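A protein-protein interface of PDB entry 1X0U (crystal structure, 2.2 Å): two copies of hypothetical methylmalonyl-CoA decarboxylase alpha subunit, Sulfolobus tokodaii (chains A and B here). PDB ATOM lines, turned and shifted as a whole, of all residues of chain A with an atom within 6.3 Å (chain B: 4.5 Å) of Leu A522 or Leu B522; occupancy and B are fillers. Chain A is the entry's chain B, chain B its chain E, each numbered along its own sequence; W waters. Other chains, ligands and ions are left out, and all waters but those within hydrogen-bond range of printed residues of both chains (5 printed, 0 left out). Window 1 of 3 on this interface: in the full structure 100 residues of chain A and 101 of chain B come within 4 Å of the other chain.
Printed residues of chain B that touch a printed residue of chain A: Asp B347, Ala B350, Arg B351, Arg B385, Lys B389, Ile B520, Pro B521 and Leu B522. Hydrophobic or aromatic side chains of chain B within 4 Å of the printed part of chain A: Ala B350, Ile B520, Pro B521 and Leu B522. Among the printed residues, 19 pairs touch across the chains. Among the printed residues, Asp or Glu carboxylates within 4 Å of a Lys or Arg side-chain nitrogen of the other chain: Asp A347 with Arg B385 (3.6 Å) and Arg A385 with Asp B347 (3.2 Å).
Of the printed residues of chain B, Trp A311 touches Arg B385. Of the printed residues of chain B, Lys A389 touches Lys B389 and Leu B522. Printed residues of chain B within 4 Å of Asn A519: Arg B351. Of chain B, only Asp B347, Ala B350, Arg B351, Lys B389 and Leu B522 come within 4 Å of Leu A522. Printed residues of chain A within 4 Å of Asp B347: Arg A385 (3.2 Å) and Leu A522 (3.9 Å). Of the printed residues of chain A, Ile B520 touches Arg A351 and Arg A354. The nearest printed residue of chain A that does not touch Asp B347 is His A386 (5.3 Å).
Arg A351 touches Ile B520, and with the chains exchanged Ile A520 touches Arg B351. Arg A351 touches Leu B522, and with the chains exchanged Leu A522 touches Arg B351. Lys A389 touches its own counterpart, Lys B389. Lys A389 touches Leu B522, and with the chains exchanged Leu A522 touches Lys B389. Positions printed for both chains: 347, 350, 351, 385, 389, 520, 521 and 522. Of the 19 pairs that touch across the chains among the printed residues, 16 have their exchanged pair printed and touching as well.
Water W3 bridges the side-chain carboxylate of Asp A347 (2.7 Å) and the guanidinium group of Arg B385 (2.8 Å). Water W4 lies within hydrogen-bond range of the side-chain carboxylate (OD1) of Asp B347 (2.7 Å), the chain-end carboxylate (O) of Leu A522 (2.7 Å), the side-chain amino group (NZ) of Lys B389 (3.0 Å) and the guanidinium group (NH1) of Arg A385 (3.4 Å). Water W5 bridges the side-chain carboxylate of Asp B347 (2.7 Å) and the guanidinium group of Arg A385 (3.1 Å). Water W2 lies within hydrogen-bond range of O of Ile B520 (2.8 Å) and NH1 of Arg A354 (2.9 Å). Water W1 bridges the backbone NH of Ile B520 and the guanidinium group of Arg A354.
The side-chain carboxylate (OD2) of Asp B347 is in salt-bridge range of the side-chain amino group (NZ) of Lys B389 (2.9 Å). NH1 of Arg A385 is in salt-bridge range of OXT of Leu A522, 2.8 Å away. The side-chain amino group (NZ) of Lys A389 lies within salt-bridge range of the chain-end carboxylate (O) of Leu A522, at 2.8 Å. The guanidinium group of Arg B385 lies within salt-bridge range of the chain-end carboxylate of Leu B522 (2.8 Å). The side-chain carboxylate of Asp A347 is in salt-bridge range of the side-chain amino group of Lys A389 (2.8 Å). ND1 of His A386 is in hydrogen-bond range of OD1 of Asp A347, at 3.3 Å.
Trp A311 touches Arg B385 (CZ2 to NH2, 3.3 Å). Ala A350 touches Leu B522 (CB to CD1, 3.9 Å). Pro B521 touches Arg A351. Leu B522 touches Arg A351 (CD1 to N, 3.8 Å). NH1 of Arg A354 touches CG2 of Ile B520, at 3.6 Å. NZ of Lys A389 touches NZ of Lys B389, 3.95 Å away. NE of Arg B351 touches CA of Pro A521, at 3.6 Å. Asp B347 touches Leu A522 (OD1 to OXT, 3.9 Å). Leu A522 touches Ala B350. Leu A522 touches Leu B522 (CD2 to CD2, 3.9 Å).
The side-chain amino group (NZ) of Lys A389 lies within salt-bridge range of the chain-end carboxylate (O) of Leu B522 (3.2 Å). O of Asn A519 lies within hydrogen-bond range of NH2 of Arg B351, 2.8 Å away. O of Leu A522 lies within salt-bridge range of NZ of Lys B389. The side-chain carboxylate (OD1) of Asp A347 lies close to the chain-end carboxylate (O) of Leu B522 (2.8 Å). The side-chain carboxylate of Asp B347 lies within salt-bridge range of the guanidinium group of Arg A385 (3.2 Å). OD2 of Asp A347 is in salt-bridge range of NH1 of Arg B385, 3.6 Å away. NE of Arg B351 lies within hydrogen-bond range of O of Ile A520 (2.9 Å). The guanidinium group (NE) of Arg A351 is in hydrogen-bond range of the backbone carbonyl oxygen (O) of Ile B520 (3.2 Å).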
ATOM      1  N   TRP A 311     -34.071  20.741  35.347  1.00  0.00           N
ATOM      2  CA  TRP A 311     -34.048  19.665  34.359  1.00  0.00           C
ATOM      3  C   TRP A 311     -33.380  18.436  34.986  1.00  0.00           C
ATOM      4  O   TRP A 311     -32.401  18.561  35.724  1.00  0.00           O
ATOM      5  CB  TRP A 311     -33.269  20.113  33.116  1.00  0.00           C
ATOM      6  CG  TRP A 311     -33.285  19.112  31.992  1.00  0.00           C
ATOM      7  CD1 TRP A 311     -34.384  18.619  31.351  1.00  0.00           C
ATOM      8  CD2 TRP A 311     -32.147  18.494  31.370  1.00  0.00           C
ATOM      9  NE1 TRP A 311     -34.006  17.735  30.370  1.00  0.00           N
ATOM     10  CE2 TRP A 311     -32.640  17.637  30.362  1.00  0.00           C
ATOM     11  CE3 TRP A 311     -30.764  18.583  31.570  1.00  0.00           C
ATOM     12  CZ2 TRP A 311     -31.792  16.865  29.549  1.00  0.00           C
ATOM     13  CZ3 TRP A 311     -29.921  17.818  30.767  1.00  0.00           C
ATOM     14  CH2 TRP A 311     -30.443  16.967  29.766  1.00  0.00           C
ATOM     15  N   ALA A 346     -28.238  11.372  33.200  1.00  0.00           N
ATOM     16  CA  ALA A 346     -26.916  10.977  32.744  1.00  0.00           C
ATOM     17  C   ALA A 346     -26.302  12.077  31.891  1.00  0.00           C
ATOM     18  O   ALA A 346     -25.107  12.359  32.015  1.00  0.00           O
ATOM     19  CB  ALA A 346     -26.992   9.669  31.951  1.00  0.00           C
ATOM     20  N   ASP A 347     -27.109  12.703  31.031  1.00  0.00           N
ATOM     21  CA  ASP A 347     -26.591  13.771  30.178  1.00  0.00           C
ATOM     22  C   ASP A 347     -26.165  14.955  31.032  1.00  0.00           C
ATOM     23  O   ASP A 347     -25.074  15.503  30.870  1.00  0.00           O
ATOM     24  CB  ASP A 347     -27.638  14.233  29.161  1.00  0.00           C
ATOM     25  CG  ASP A 347     -27.819  13.253  28.009  1.00  0.00           C
ATOM     26  OD1 ASP A 347     -26.850  12.552  27.647  1.00  0.00           O
ATOM     27  OD2 ASP A 347     -28.928  13.201  27.444  1.00  0.00           O
ATOM     28  N   LYS A 348     -27.034  15.333  31.957  1.00  0.00           N
ATOM     29  CA  LYS A 348     -26.767  16.446  32.855  1.00  0.00           C
ATOM     30  C   LYS A 348     -25.476  16.248  33.653  1.00  0.00           C
ATOM     31  O   LYS A 348     -24.598  17.108  33.651  1.00  0.00           O
ATOM     32  CB  LYS A 348     -27.957  16.607  33.805  1.00  0.00           C
ATOM     33  CG  LYS A 348     -27.772  17.587  34.944  1.00  0.00           C
ATOM     34  CD  LYS A 348     -29.067  17.645  35.737  1.00  0.00           C
ATOM     35  CE  LYS A 348     -28.944  18.508  36.964  1.00  0.00           C
ATOM     36  NZ  LYS A 348     -30.156  18.380  37.818  1.00  0.00           N
ATOM     37  N   ALA A 350     -22.938  13.977  33.209  1.00  0.00           N
ATOM     38  CA  ALA A 350     -21.757  13.755  32.385  1.00  0.00           C
ATOM     39  C   ALA A 350     -21.161  15.048  31.849  1.00  0.00           C
ATOM     40  O   ALA A 350     -19.943  15.241  31.905  1.00  0.00           O
ATOM     41  CB  ALA A 350     -22.086  12.817  31.235  1.00  0.00           C
ATOM     42  N   ARG A 351     -22.026  15.915  31.328  1.00  0.00           N
ATOM     43  CA  ARG A 351     -21.608  17.189  30.778  1.00  0.00           C
ATOM     44  C   ARG A 351     -20.931  17.981  31.894  1.00  0.00           C
ATOM     45  O   ARG A 351     -19.828  18.491  31.718  1.00  0.00           O
ATOM     46  CB  ARG A 351     -22.827  17.954  30.229  1.00  0.00           C
ATOM     47  CG  ARG A 351     -22.682  18.516  28.790  1.00  0.00           C
ATOM     48  CD  ARG A 351     -21.551  19.507  28.709  1.00  0.00           C
ATOM     49  NE  ARG A 351     -21.352  20.171  27.411  1.00  0.00           N
ATOM     50  CZ  ARG A 351     -22.037  21.229  26.971  1.00  0.00           C
ATOM     51  NH1 ARG A 351     -23.011  21.759  27.703  1.00  0.00           N
ATOM     52  NH2 ARG A 351     -21.683  21.823  25.837  1.00  0.00           N
ATOM     53  N   ARG A 354     -17.467  16.622  32.751  1.00  0.00           N
ATOM     54  CA  ARG A 354     -16.431  16.900  31.766  1.00  0.00           C
ATOM     55  C   ARG A 354     -15.974  18.364  31.798  1.00  0.00           C
ATOM     56  O   ARG A 354     -14.811  18.666  31.516  1.00  0.00           O
ATOM     57  CB  ARG A 354     -16.919  16.530  30.367  1.00  0.00           C
ATOM     58  CG  ARG A 354     -17.268  15.059  30.201  1.00  0.00           C
ATOM     59  CD  ARG A 354     -17.362  14.708  28.721  1.00  0.00           C
ATOM     60  NE  ARG A 354     -16.050  14.645  28.088  1.00  0.00           N
ATOM     61  CZ  ARG A 354     -15.788  15.074  26.857  1.00  0.00           C
ATOM     62  NH1 ARG A 354     -16.747  15.607  26.121  1.00  0.00           N
ATOM     63  NH2 ARG A 354     -14.564  14.961  26.353  1.00  0.00           N
ATOM     64  N   ARG A 385     -26.490   3.946  25.788  1.00  0.00           N
ATOM     65  CA  ARG A 385     -25.452   4.885  25.397  1.00  0.00           C
ATOM     66  C   ARG A 385     -25.417   6.181  26.207  1.00  0.00           C
ATOM     67  O   ARG A 385     -24.355   6.785  26.356  1.00  0.00           O
ATOM     68  CB  ARG A 385     -25.558   5.210  23.900  1.00  0.00           C
ATOM     69  CG  ARG A 385     -26.808   5.939  23.461  1.00  0.00           C
ATOM     70  CD  ARG A 385     -26.797   6.078  21.943  1.00  0.00           C
ATOM     71  NE  ARG A 385     -28.143   6.255  21.412  1.00  0.00           N
ATOM     72  CZ  ARG A 385     -28.712   7.427  21.161  1.00  0.00           C
ATOM     73  NH1 ARG A 385     -28.053   8.561  21.373  1.00  0.00           N
ATOM     74  NH2 ARG A 385     -29.958   7.459  20.717  1.00  0.00           N
ATOM     75  N   HIS A 386     -26.564   6.613  26.726  1.00  0.00           N
ATOM     76  CA  HIS A 386     -26.616   7.840  27.519  1.00  0.00           C
ATOM     77  C   HIS A 386     -25.999   7.581  28.878  1.00  0.00           C
ATOM     78  O   HIS A 386     -25.180   8.360  29.362  1.00  0.00           O
ATOM     79  CB  HIS A 386     -28.067   8.305  27.705  1.00  0.00           C
ATOM     80  CG  HIS A 386     -28.699   8.855  26.464  1.00  0.00           C
ATOM     81  ND1 HIS A 386     -28.501  10.150  26.040  1.00  0.00           N
ATOM     82  CD2 HIS A 386     -29.527   8.284  25.555  1.00  0.00           C
ATOM     83  CE1 HIS A 386     -29.179  10.356  24.926  1.00  0.00           C
ATOM     84  NE2 HIS A 386     -29.808   9.239  24.609  1.00  0.00           N
ATOM     85  N   LYS A 389     -22.272   7.665  29.190  1.00  0.00           N
ATOM     86  CA  LYS A 389     -21.604   8.965  29.205  1.00  0.00           C
ATOM     87  C   LYS A 389     -21.008   9.326  30.577  1.00  0.00           C
ATOM     88  O   LYS A 389     -19.927   9.897  30.645  1.00  0.00           O
ATOM     89  CB  LYS A 389     -22.570  10.065  28.755  1.00  0.00           C
ATOM     90  CG  LYS A 389     -23.038   9.938  27.308  1.00  0.00           C
ATOM     91  CD  LYS A 389     -24.034  11.031  26.958  1.00  0.00           C
ATOM     92  CE  LYS A 389     -24.612  10.847  25.579  1.00  0.00           C
ATOM     93  NZ  LYS A 389     -25.627  11.899  25.269  1.00  0.00           N
ATOM     94  N   ALA A 393     -17.224   9.943  31.378  1.00  0.00           N
ATOM     95  CA  ALA A 393     -16.883  11.214  32.022  1.00  0.00           C
ATOM     96  C   ALA A 393     -16.001  11.053  33.263  1.00  0.00           C
ATOM     97  O   ALA A 393     -14.945  11.681  33.359  1.00  0.00           O
ATOM     98  CB  ALA A 393     -18.179  11.995  32.373  1.00  0.00           C
ATOM     99  N   ASN A 519     -13.889   8.846  21.933  1.00  0.00           N
ATOM    100  CA  ASN A 519     -15.098   8.678  21.145  1.00  0.00           C
ATOM    101  C   ASN A 519     -16.263   8.376  22.065  1.00  0.00           C
ATOM    102  O   ASN A 519     -16.913   7.340  21.941  1.00  0.00           O
ATOM    103  CB  ASN A 519     -14.908   7.541  20.138  1.00  0.00           C
ATOM    104  CG  ASN A 519     -16.100   7.367  19.232  1.00  0.00           C
ATOM    105  OD1 ASN A 519     -16.753   8.342  18.853  1.00  0.00           O
ATOM    106  ND2 ASN A 519     -16.387   6.125  18.866  1.00  0.00           N
ATOM    107  N   ILE A 520     -16.517   9.289  22.993  1.00  0.00           N
ATOM    108  CA  ILE A 520     -17.599   9.119  23.958  1.00  0.00           C
ATOM    109  C   ILE A 520     -18.957   8.847  23.301  1.00  0.00           C
ATOM    110  O   ILE A 520     -19.235   9.323  22.201  1.00  0.00           O
ATOM    111  CB  ILE A 520     -17.709  10.376  24.853  1.00  0.00           C
ATOM    112  CG1 ILE A 520     -18.786  10.181  25.918  1.00  0.00           C
ATOM    113  CG2 ILE A 520     -18.022  11.598  23.995  1.00  0.00           C
ATOM    114  CD1 ILE A 520     -18.706  11.201  27.026  1.00  0.00           C
ATOM    115  N   PRO A 521     -19.814   8.046  23.953  1.00  0.00           N
ATOM    116  CA  PRO A 521     -21.122   7.798  23.327  1.00  0.00           C
ATOM    117  C   PRO A 521     -21.888   9.129  23.209  1.00  0.00           C
ATOM    118  O   PRO A 521     -21.842   9.961  24.120  1.00  0.00           O
ATOM    119  CB  PRO A 521     -21.797   6.837  24.305  1.00  0.00           C
ATOM    120  CG  PRO A 521     -20.647   6.086  24.887  1.00  0.00           C
ATOM    121  CD  PRO A 521     -19.623   7.178  25.128  1.00  0.00           C
ATOM    122  N   LEU A 522     -22.585   9.331  22.097  1.00  0.00           N
ATOM    123  CA  LEU A 522     -23.343  10.567  21.903  1.00  0.00           C
ATOM    124  C   LEU A 522     -24.862  10.366  21.989  1.00  0.00           C
ATOM    125  O   LEU A 522     -25.546  11.220  22.593  1.00  0.00           O
ATOM    126  CB  LEU A 522     -22.958  11.222  20.566  1.00  0.00           C
ATOM    127  CG  LEU A 522     -21.509  11.729  20.495  1.00  0.00           C
ATOM    128  CD1 LEU A 522     -21.255  12.500  19.208  1.00  0.00           C
ATOM    129  CD2 LEU A 522     -21.245  12.626  21.690  1.00  0.00           C
ATOM    130  OXT LEU A 522     -25.361   9.357  21.455  1.00  0.00           O
ATOM    131  N   ASP B 347     -26.897  12.598  16.044  1.00  0.00           N
ATOM    132  CA  ASP B 347     -26.110  11.722  16.908  1.00  0.00           C
ATOM    133  C   ASP B 347     -25.336  10.714  16.063  1.00  0.00           C
ATOM    134  O   ASP B 347     -24.142  10.515  16.231  1.00  0.00           O
ATOM    135  CB  ASP B 347     -27.020  10.962  17.876  1.00  0.00           C
ATOM    136  CG  ASP B 347     -27.440  11.802  19.053  1.00  0.00           C
ATOM    137  OD1 ASP B 347     -28.296  11.344  19.827  1.00  0.00           O
ATOM    138  OD2 ASP B 347     -26.904  12.919  19.212  1.00  0.00           O
ATOM    139  N   ALA B 350     -22.565  12.577  13.966  1.00  0.00           N
ATOM    140  CA  ALA B 350     -21.550  13.159  14.837  1.00  0.00           C
ATOM    141  C   ALA B 350     -20.537  12.144  15.375  1.00  0.00           C
ATOM    142  O   ALA B 350     -19.333  12.378  15.292  1.00  0.00           O
ATOM    143  CB  ALA B 350     -22.215  13.909  15.987  1.00  0.00           C
ATOM    144  N   ARG B 351     -21.011  11.025  15.921  1.00  0.00           N
ATOM    145  CA  ARG B 351     -20.100  10.011  16.465  1.00  0.00           C
ATOM    146  C   ARG B 351     -19.271   9.341  15.375  1.00  0.00           C
ATOM    147  O   ARG B 351     -18.123   8.981  15.607  1.00  0.00           O
ATOM    148  CB  ARG B 351     -20.871   8.941  17.248  1.00  0.00           C
ATOM    149  CG  ARG B 351     -19.969   7.948  17.996  1.00  0.00           C
ATOM    150  CD  ARG B 351     -20.313   7.938  19.483  1.00  0.00           C
ATOM    151  NE  ARG B 351     -19.399   7.123  20.288  1.00  0.00           N
ATOM    152  CZ  ARG B 351     -19.542   5.817  20.521  1.00  0.00           C
ATOM    153  NH1 ARG B 351     -20.573   5.140  20.015  1.00  0.00           N
ATOM    154  NH2 ARG B 351     -18.646   5.182  21.267  1.00  0.00           N
ATOM    155  N   ARG B 385     -29.074  21.070  21.147  1.00  0.00           N
ATOM    156  CA  ARG B 385     -27.829  20.484  21.617  1.00  0.00           C
ATOM    157  C   ARG B 385     -27.382  19.300  20.774  1.00  0.00           C
ATOM    158  O   ARG B 385     -26.193  19.147  20.504  1.00  0.00           O
ATOM    159  CB  ARG B 385     -27.921  20.092  23.101  1.00  0.00           C
ATOM    160  CG  ARG B 385     -29.039  19.149  23.518  1.00  0.00           C
ATOM    161  CD  ARG B 385     -29.110  19.134  25.055  1.00  0.00           C
ATOM    162  NE  ARG B 385     -30.231  18.371  25.579  1.00  0.00           N
ATOM    163  CZ  ARG B 385     -30.189  17.075  25.872  1.00  0.00           C
ATOM    164  NH1 ARG B 385     -29.072  16.376  25.707  1.00  0.00           N
ATOM    165  NH2 ARG B 385     -31.283  16.467  26.298  1.00  0.00           N
ATOM    166  N   LYS B 389     -23.829  18.699  17.818  1.00  0.00           N
ATOM    167  CA  LYS B 389     -22.777  17.689  17.886  1.00  0.00           C
ATOM    168  C   LYS B 389     -22.070  17.522  16.540  1.00  0.00           C
ATOM    169  O   LYS B 389     -20.874  17.244  16.495  1.00  0.00           O
ATOM    170  CB  LYS B 389     -23.355  16.351  18.357  1.00  0.00           C
ATOM    171  CG  LYS B 389     -23.811  16.335  19.826  1.00  0.00           C
ATOM    172  CD  LYS B 389     -24.566  15.049  20.149  1.00  0.00           C
ATOM    173  CE  LYS B 389     -25.060  15.010  21.592  1.00  0.00           C
ATOM    174  NZ  LYS B 389     -25.928  13.823  21.828  1.00  0.00           N
ATOM    175  N   ILE B 520     -17.909  18.891  24.291  1.00  0.00           N
ATOM    176  CA  ILE B 520     -18.978  18.743  23.314  1.00  0.00           C
ATOM    177  C   ILE B 520     -20.358  18.616  23.963  1.00  0.00           C
ATOM    178  O   ILE B 520     -20.491  18.094  25.065  1.00  0.00           O
ATOM    179  CB  ILE B 520     -18.736  17.503  22.412  1.00  0.00           C
ATOM    180  CG1 ILE B 520     -19.743  17.495  21.261  1.00  0.00           C
ATOM    181  CG2 ILE B 520     -18.842  16.228  23.239  1.00  0.00           C
ATOM    182  CD1 ILE B 520     -19.340  16.642  20.078  1.00  0.00           C
ATOM    183  N   PRO B 521     -21.398  19.135  23.295  1.00  0.00           N
ATOM    184  CA  PRO B 521     -22.760  19.045  23.839  1.00  0.00           C
ATOM    185  C   PRO B 521     -23.139  17.565  23.957  1.00  0.00           C
ATOM    186  O   PRO B 521     -22.872  16.791  23.048  1.00  0.00           O
ATOM    187  CB  PRO B 521     -23.604  19.751  22.772  1.00  0.00           C
ATOM    188  CG  PRO B 521     -22.668  20.785  22.218  1.00  0.00           C
ATOM    189  CD  PRO B 521     -21.341  20.053  22.139  1.00  0.00           C
ATOM    190  N   LEU B 522     -23.757  17.172  25.065  1.00  0.00           N
ATOM    191  CA  LEU B 522     -24.180  15.785  25.242  1.00  0.00           C
ATOM    192  C   LEU B 522     -25.700  15.695  25.407  1.00  0.00           C
ATOM    193  O   LEU B 522     -26.141  14.925  26.284  1.00  0.00           O
ATOM    194  CB  LEU B 522     -23.514  15.169  26.474  1.00  0.00           C
ATOM    195  CG  LEU B 522     -21.985  15.044  26.468  1.00  0.00           C
ATOM    196  CD1 LEU B 522     -21.518  14.484  27.804  1.00  0.00           C
ATOM    197  CD2 LEU B 522     -21.547  14.146  25.315  1.00  0.00           C
ATOM    198  OXT LEU B 522     -26.434  16.380  24.671  1.00  0.00           O
HETATM  199  O   HOH W   1     -15.522  17.145  23.502  1.00  0.00           O
HETATM  200  O   HOH W   2     -18.938  17.091  27.232  1.00  0.00           O
HETATM  201  O   HOH W   3     -31.472  13.811  27.019  1.00  0.00           O
HETATM  202  O   HOH W   4     -28.130  11.824  22.434  1.00  0.00           O
HETATM  203  O   HOH W   5     -30.786  10.210  19.665  1.00  0.00           O
